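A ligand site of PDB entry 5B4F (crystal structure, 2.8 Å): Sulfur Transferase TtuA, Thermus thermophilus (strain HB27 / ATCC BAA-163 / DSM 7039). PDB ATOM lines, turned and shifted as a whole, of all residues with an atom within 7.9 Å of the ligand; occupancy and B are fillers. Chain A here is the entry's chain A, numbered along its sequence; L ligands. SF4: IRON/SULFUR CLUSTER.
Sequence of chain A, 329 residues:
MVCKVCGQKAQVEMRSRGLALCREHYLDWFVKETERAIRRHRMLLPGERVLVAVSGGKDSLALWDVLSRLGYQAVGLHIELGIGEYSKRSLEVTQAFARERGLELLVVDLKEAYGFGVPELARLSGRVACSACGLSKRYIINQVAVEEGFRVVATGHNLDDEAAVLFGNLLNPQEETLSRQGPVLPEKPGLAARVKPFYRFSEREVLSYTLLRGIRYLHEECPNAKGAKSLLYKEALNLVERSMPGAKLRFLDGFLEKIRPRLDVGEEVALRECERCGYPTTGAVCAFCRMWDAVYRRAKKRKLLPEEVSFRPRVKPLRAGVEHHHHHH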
ATOM      1  N   SER A  55     -26.446   8.926  -9.365  1.00  0.00           N
ATOM      2  CA  SER A  55     -25.128   8.624  -8.805  1.00  0.00           C
ATOM      3  C   SER A  55     -25.133   7.553  -7.750  1.00  0.00           C
ATOM      4  O   SER A  55     -24.093   6.965  -7.467  1.00  0.00           O
ATOM      5  CB  SER A  55     -24.529   9.872  -8.169  1.00  0.00           C
ATOM      6  OG  SER A  55     -25.399  10.364  -7.157  1.00  0.00           O
ATOM      7  N   LEU A  81     -17.385   5.685 -12.975  1.00  0.00           N
ATOM      8  CA  LEU A  81     -16.304   6.597 -13.358  1.00  0.00           C
ATOM      9  C   LEU A  81     -14.915   6.023 -13.128  1.00  0.00           C
ATOM     10  O   LEU A  81     -13.912   6.654 -13.483  1.00  0.00           O
ATOM     11  CB  LEU A  81     -16.448   7.926 -12.600  1.00  0.00           C
ATOM     12  CG  LEU A  81     -17.729   8.664 -13.016  1.00  0.00           C
ATOM     13  CD1 LEU A  81     -18.082   9.786 -12.049  1.00  0.00           C
ATOM     14  CD2 LEU A  81     -17.589   9.206 -14.422  1.00  0.00           C
ATOM     15  N   ILE A  83     -13.390   5.366 -10.214  1.00  0.00           N
ATOM     16  CA  ILE A  83     -12.687   5.936  -9.064  1.00  0.00           C
ATOM     17  C   ILE A  83     -12.695   4.935  -7.901  1.00  0.00           C
ATOM     18  O   ILE A  83     -13.369   5.118  -6.886  1.00  0.00           O
ATOM     19  CB  ILE A  83     -13.330   7.283  -8.632  1.00  0.00           C
ATOM     20  CG1 ILE A  83     -13.408   8.224  -9.828  1.00  0.00           C
ATOM     21  CG2 ILE A  83     -12.533   7.911  -7.483  1.00  0.00           C
ATOM     22  CD1 ILE A  83     -14.371   9.388  -9.667  1.00  0.00           C
ATOM     23  N   TYR A  86     -14.924   3.588  -4.288  1.00  0.00           N
ATOM     24  CA  TYR A  86     -15.990   4.581  -4.431  1.00  0.00           C
ATOM     25  C   TYR A  86     -16.915   4.339  -5.639  1.00  0.00           C
ATOM     26  O   TYR A  86     -18.145   4.296  -5.491  1.00  0.00           O
ATOM     27  CB  TYR A  86     -15.403   5.978  -4.532  1.00  0.00           C
ATOM     28  CG  TYR A  86     -16.474   7.022  -4.791  1.00  0.00           C
ATOM     29  CD1 TYR A  86     -17.361   7.394  -3.787  1.00  0.00           C
ATOM     30  CD2 TYR A  86     -16.613   7.612  -6.038  1.00  0.00           C
ATOM     31  CE1 TYR A  86     -18.352   8.335  -4.007  1.00  0.00           C
ATOM     32  CE2 TYR A  86     -17.597   8.559  -6.269  1.00  0.00           C
ATOM     33  CZ  TYR A  86     -18.463   8.916  -5.249  1.00  0.00           C
ATOM     34  OH  TYR A  86     -19.442   9.854  -5.481  1.00  0.00           O
ATOM     35  N   SER A  87     -16.328   4.199  -6.830  1.00  0.00           N
ATOM     36  CA  SER A  87     -17.175   4.028  -8.023  1.00  0.00           C
ATOM     37  C   SER A  87     -17.844   2.673  -7.956  1.00  0.00           C
ATOM     38  O   SER A  87     -18.979   2.510  -8.433  1.00  0.00           O
ATOM     39  CB  SER A  87     -16.377   4.179  -9.313  1.00  0.00           C
ATOM     40  OG  SER A  87     -15.885   5.512  -9.445  1.00  0.00           O
ATOM     41  N   VAL A 118     -11.526   7.948 -14.596  1.00  0.00           N
ATOM     42  CA  VAL A 118     -11.289   9.331 -14.237  1.00  0.00           C
ATOM     43  C   VAL A 118      -9.872   9.600 -13.683  1.00  0.00           C
ATOM     44  O   VAL A 118      -9.285  10.648 -13.988  1.00  0.00           O
ATOM     45  CB  VAL A 118     -12.347   9.818 -13.216  1.00  0.00           C
ATOM     46  CG1 VAL A 118     -11.935  11.141 -12.576  1.00  0.00           C
ATOM     47  CG2 VAL A 118     -13.716   9.932 -13.887  1.00  0.00           C
ATOM     48  N   PRO A 119      -9.315   8.681 -12.866  1.00  0.00           N
ATOM     49  CA  PRO A 119      -7.956   9.018 -12.418  1.00  0.00           C
ATOM     50  C   PRO A 119      -6.954   9.157 -13.558  1.00  0.00           C
ATOM     51  O   PRO A 119      -6.327  10.214 -13.665  1.00  0.00           O
ATOM     52  CB  PRO A 119      -7.574   7.847 -11.504  1.00  0.00           C
ATOM     53  CG  PRO A 119      -8.908   7.341 -10.994  1.00  0.00           C
ATOM     54  CD  PRO A 119      -9.858   7.507 -12.142  1.00  0.00           C
ATOM     55  N   VAL A 128      -7.661  18.783 -13.843  1.00  0.00           N
ATOM     56  CA  VAL A 128      -7.969  18.240 -12.531  1.00  0.00           C
ATOM     57  C   VAL A 128      -9.085  17.212 -12.712  1.00  0.00           C
ATOM     58  O   VAL A 128      -9.984  17.388 -13.561  1.00  0.00           O
ATOM     59  CB  VAL A 128      -8.410  19.344 -11.522  1.00  0.00           C
ATOM     60  CG1 VAL A 128      -7.263  20.269 -11.235  1.00  0.00           C
ATOM     61  CG2 VAL A 128      -9.610  20.143 -12.057  1.00  0.00           C
ATOM     62  N   ALA A 129      -8.997  16.142 -11.935  1.00  0.00           N
ATOM     63  CA  ALA A 129      -9.945  15.039 -11.975  1.00  0.00           C
ATOM     64  C   ALA A 129     -11.423  15.475 -12.123  1.00  0.00           C
ATOM     65  O   ALA A 129     -12.175  14.901 -12.919  1.00  0.00           O
ATOM     66  CB  ALA A 129      -9.787  14.191 -10.754  1.00  0.00           C
ATOM     67  N   CYS A 130     -11.824  16.509 -11.390  1.00  0.00           N
ATOM     68  CA  CYS A 130     -13.225  16.930 -11.419  1.00  0.00           C
ATOM     69  C   CYS A 130     -13.571  17.649 -12.704  1.00  0.00           C
ATOM     70  O   CYS A 130     -14.734  17.613 -13.145  1.00  0.00           O
ATOM     71  CB  CYS A 130     -13.554  17.819 -10.203  1.00  0.00           C
ATOM     72  SG  CYS A 130     -13.246  17.027  -8.593  1.00  0.00           S
ATOM     73  N   SER A 131     -12.572  18.297 -13.311  1.00  0.00           N
ATOM     74  CA  SER A 131     -12.776  18.911 -14.627  1.00  0.00           C
ATOM     75  C   SER A 131     -12.983  17.858 -15.724  1.00  0.00           C
ATOM     76  O   SER A 131     -13.912  17.967 -16.534  1.00  0.00           O
ATOM     77  CB  SER A 131     -11.588  19.817 -14.987  1.00  0.00           C
ATOM     78  OG  SER A 131     -11.890  20.561 -16.155  1.00  0.00           O
ATOM     79  N   ALA A 132     -12.126  16.842 -15.733  1.00  0.00           N
ATOM     80  CA  ALA A 132     -12.256  15.758 -16.682  1.00  0.00           C
ATOM     81  C   ALA A 132     -13.555  15.042 -16.440  1.00  0.00           C
ATOM     82  O   ALA A 132     -14.334  14.795 -17.376  1.00  0.00           O
ATOM     83  CB  ALA A 132     -11.096  14.795 -16.572  1.00  0.00           C
ATOM     84  N   CYS A 133     -13.796  14.753 -15.158  1.00  0.00           N
ATOM     85  CA  CYS A 133     -14.987  14.018 -14.742  1.00  0.00           C
ATOM     86  C   CYS A 133     -16.288  14.736 -15.034  1.00  0.00           C
ATOM     87  O   CYS A 133     -17.209  14.158 -15.632  1.00  0.00           O
ATOM     88  CB  CYS A 133     -14.906  13.721 -13.257  1.00  0.00           C
ATOM     89  SG  CYS A 133     -16.256  12.718 -12.666  1.00  0.00           S
ATOM     90  N   GLY A 134     -16.350  16.000 -14.660  1.00  0.00           N
ATOM     91  CA  GLY A 134     -17.533  16.786 -14.995  1.00  0.00           C
ATOM     92  C   GLY A 134     -17.850  16.840 -16.485  1.00  0.00           C
ATOM     93  O   GLY A 134     -19.022  16.672 -16.906  1.00  0.00           O
ATOM     94  N   LEU A 135     -16.820  17.083 -17.285  1.00  0.00           N
ATOM     95  CA  LEU A 135     -16.978  17.122 -18.740  1.00  0.00           C
ATOM     96  C   LEU A 135     -17.451  15.747 -19.254  1.00  0.00           C
ATOM     97  O   LEU A 135     -18.359  15.651 -20.127  1.00  0.00           O
ATOM     98  CB  LEU A 135     -15.647  17.544 -19.368  1.00  0.00           C
ATOM     99  CG  LEU A 135     -15.554  17.458 -20.884  1.00  0.00           C
ATOM    100  CD1 LEU A 135     -16.810  18.040 -21.510  1.00  0.00           C
ATOM    101  CD2 LEU A 135     -14.283  18.148 -21.398  1.00  0.00           C
ATOM    102  N   LYS A 137     -19.056  13.447 -17.549  1.00  0.00           N
ATOM    103  CA  LYS A 137     -20.435  13.204 -17.132  1.00  0.00           C
ATOM    104  C   LYS A 137     -21.449  13.962 -18.014  1.00  0.00           C
ATOM    105  O   LYS A 137     -22.430  13.354 -18.483  1.00  0.00           O
ATOM    106  CB  LYS A 137     -20.623  13.554 -15.649  1.00  0.00           C
ATOM    107  CG  LYS A 137     -20.000  12.534 -14.709  1.00  0.00           C
ATOM    108  CD  LYS A 137     -20.150  12.938 -13.238  1.00  0.00           C
ATOM    109  CE  LYS A 137     -19.600  14.318 -12.938  1.00  0.00           C
ATOM    110  NZ  LYS A 137     -19.558  14.548 -11.472  1.00  0.00           N
ATOM    111  N   GLU A 221     -18.617  10.086   0.313  1.00  0.00           N
ATOM    112  CA  GLU A 221     -18.408  11.070  -0.751  1.00  0.00           C
ATOM    113  C   GLU A 221     -17.165  10.724  -1.585  1.00  0.00           C
ATOM    114  O   GLU A 221     -16.339   9.897  -1.187  1.00  0.00           O
ATOM    115  CB  GLU A 221     -18.306  12.474  -0.176  1.00  0.00           C
ATOM    116  CG  GLU A 221     -17.241  12.637   0.901  1.00  0.00           C
ATOM    117  CD  GLU A 221     -17.302  14.003   1.558  1.00  0.00           C
ATOM    118  OE1 GLU A 221     -16.269  14.464   2.108  1.00  0.00           O
ATOM    119  OE2 GLU A 221     -18.396  14.599   1.538  1.00  0.00           O
ATOM    120  N   CYS A 222     -17.038  11.344  -2.749  1.00  0.00           N
ATOM    121  CA  CYS A 222     -15.922  11.018  -3.613  1.00  0.00           C
ATOM    122  C   CYS A 222     -14.599  11.550  -3.082  1.00  0.00           C
ATOM    123  O   CYS A 222     -14.503  12.726  -2.719  1.00  0.00           O
ATOM    124  CB  CYS A 222     -16.162  11.551  -5.022  1.00  0.00           C
ATOM    125  SG  CYS A 222     -14.819  11.172  -6.240  1.00  0.00           S
ATOM    126  N   PRO A 223     -13.553  10.694  -3.076  1.00  0.00           N
ATOM    127  CA  PRO A 223     -12.209  11.020  -2.608  1.00  0.00           C
ATOM    128  C   PRO A 223     -11.720  12.409  -3.019  1.00  0.00           C
ATOM    129  O   PRO A 223     -11.156  13.110  -2.193  1.00  0.00           O
ATOM    130  CB  PRO A 223     -11.340   9.934  -3.245  1.00  0.00           C
ATOM    131  CG  PRO A 223     -12.238   8.780  -3.379  1.00  0.00           C
ATOM    132  CD  PRO A 223     -13.643   9.306  -3.570  1.00  0.00           C
ATOM    133  N   ASN A 224     -11.911  12.792  -4.266  1.00  0.00           N
ATOM    134  CA  ASN A 224     -11.655  14.187  -4.601  1.00  0.00           C
ATOM    135  C   ASN A 224     -12.906  14.817  -5.163  1.00  0.00           C
ATOM    136  O   ASN A 224     -13.394  14.366  -6.172  1.00  0.00           O
ATOM    137  CB  ASN A 224     -10.486  14.364  -5.601  1.00  0.00           C
ATOM    138  CG  ASN A 224     -10.416  13.263  -6.663  1.00  0.00           C
ATOM    139  OD1 ASN A 224      -9.339  12.712  -6.900  1.00  0.00           O
ATOM    140  ND2 ASN A 224     -11.530  12.959  -7.318  1.00  0.00           N
ATOM    141  N   ALA A 225     -13.370  15.883  -4.539  1.00  0.00           N
ATOM    142  CA  ALA A 225     -12.640  16.574  -3.495  1.00  0.00           C
ATOM    143  C   ALA A 225     -13.655  16.925  -2.412  1.00  0.00           C
ATOM    144  O   ALA A 225     -14.844  17.006  -2.748  1.00  0.00           O
ATOM    145  CB  ALA A 225     -11.935  17.817  -4.076  1.00  0.00           C
ATOM    146  N   LYS A 226     -13.288  17.101  -1.133  1.00  0.00           N
ATOM    147  CA  LYS A 226     -11.955  17.118  -0.477  1.00  0.00           C
ATOM    148  C   LYS A 226     -11.102  18.294  -0.954  1.00  0.00           C
ATOM    149  O   LYS A 226      -9.916  18.155  -1.232  1.00  0.00           O
ATOM    150  CB  LYS A 226     -11.203  15.792  -0.639  1.00  0.00           C
ATOM    151  CG  LYS A 226     -10.160  15.523   0.454  1.00  0.00           C
ATOM    152  CD  LYS A 226     -10.800  15.302   1.825  1.00  0.00           C
ATOM    153  CE  LYS A 226      -9.771  14.920   2.880  1.00  0.00           C
ATOM    154  NZ  LYS A 226     -10.376  14.718   4.237  1.00  0.00           N
ATOM    155  N   ALA A 228     -13.237  20.756  -2.619  1.00  0.00           N
ATOM    156  CA  ALA A 228     -14.192  21.246  -3.615  1.00  0.00           C
ATOM    157  C   ALA A 228     -14.469  22.719  -3.382  1.00  0.00           C
ATOM    158  O   ALA A 228     -14.562  23.162  -2.241  1.00  0.00           O
ATOM    159  CB  ALA A 228     -15.493  20.432  -3.544  1.00  0.00           C
ATOM    160  N   SER A 230     -17.260  24.156  -4.537  1.00  0.00           N
ATOM    161  CA  SER A 230     -18.683  24.066  -4.210  1.00  0.00           C
ATOM    162  C   SER A 230     -18.953  23.838  -2.705  1.00  0.00           C
ATOM    163  O   SER A 230     -19.873  24.422  -2.124  1.00  0.00           O
ATOM    164  CB  SER A 230     -19.334  22.946  -5.020  1.00  0.00           C
ATOM    165  OG  SER A 230     -18.570  21.756  -4.949  1.00  0.00           O
HETATM  166 FE1  SF4 L   1     -15.444  12.850  -7.672  1.00  0.00          FE
HETATM  167 FE2  SF4 L   1     -17.842  14.572  -8.334  1.00  0.00          FE
HETATM  168 FE3  SF4 L   1     -16.128  13.370 -10.486  1.00  0.00          FE
HETATM  169 FE4  SF4 L   1     -14.934  15.502  -8.809  1.00  0.00          FE
HETATM  170  S1  SF4 L   1     -16.728  15.364 -10.003  1.00  0.00           S
HETATM  171  S2  SF4 L   1     -14.311  13.533  -9.373  1.00  0.00           S
HETATM  172  S3  SF4 L   1     -16.084  14.803  -7.126  1.00  0.00           S
HETATM  173  S4  SF4 L   1     -17.227  12.551  -8.811  1.00  0.00           S
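The side-chain sulfur (SG) of Cys 222 lies close to the backbone carbonyl oxygen (O) of Asn 224, 3.5 Å away.
The side-chain sulfur (SG) of Cys 130 lies close to the backbone carbonyl oxygen (O) of Asn 224, 3.6 Å away.
Residues that only touch the ligand: Ala 225.
Within 4 Å of the ligand: Cys 130, Cys 133, Lys 137, Cys 222, Asn 224 and Ala 225.
A sulfur (S1) of the ligand lies close to the side-chain amino group (NZ) of Lys 137, at 3.3 Å.
The side-chain sulfur of Cys 222 is bound to an iron atom (FE1) of the ligand, 2.3 Å away.
The side-chain amide nitrogen (ND2) of Asn 224 lies close to a sulfur (S2) of the ligand (3.5 Å).
The side-chain sulfur (SG) of Cys 133 is bound to an iron atom (FE3) of the ligand (2.3 Å).
An iron atom (FE4) of the ligand is bound by the side-chain sulfur (SG) of Cys 130 (2.3 Å).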
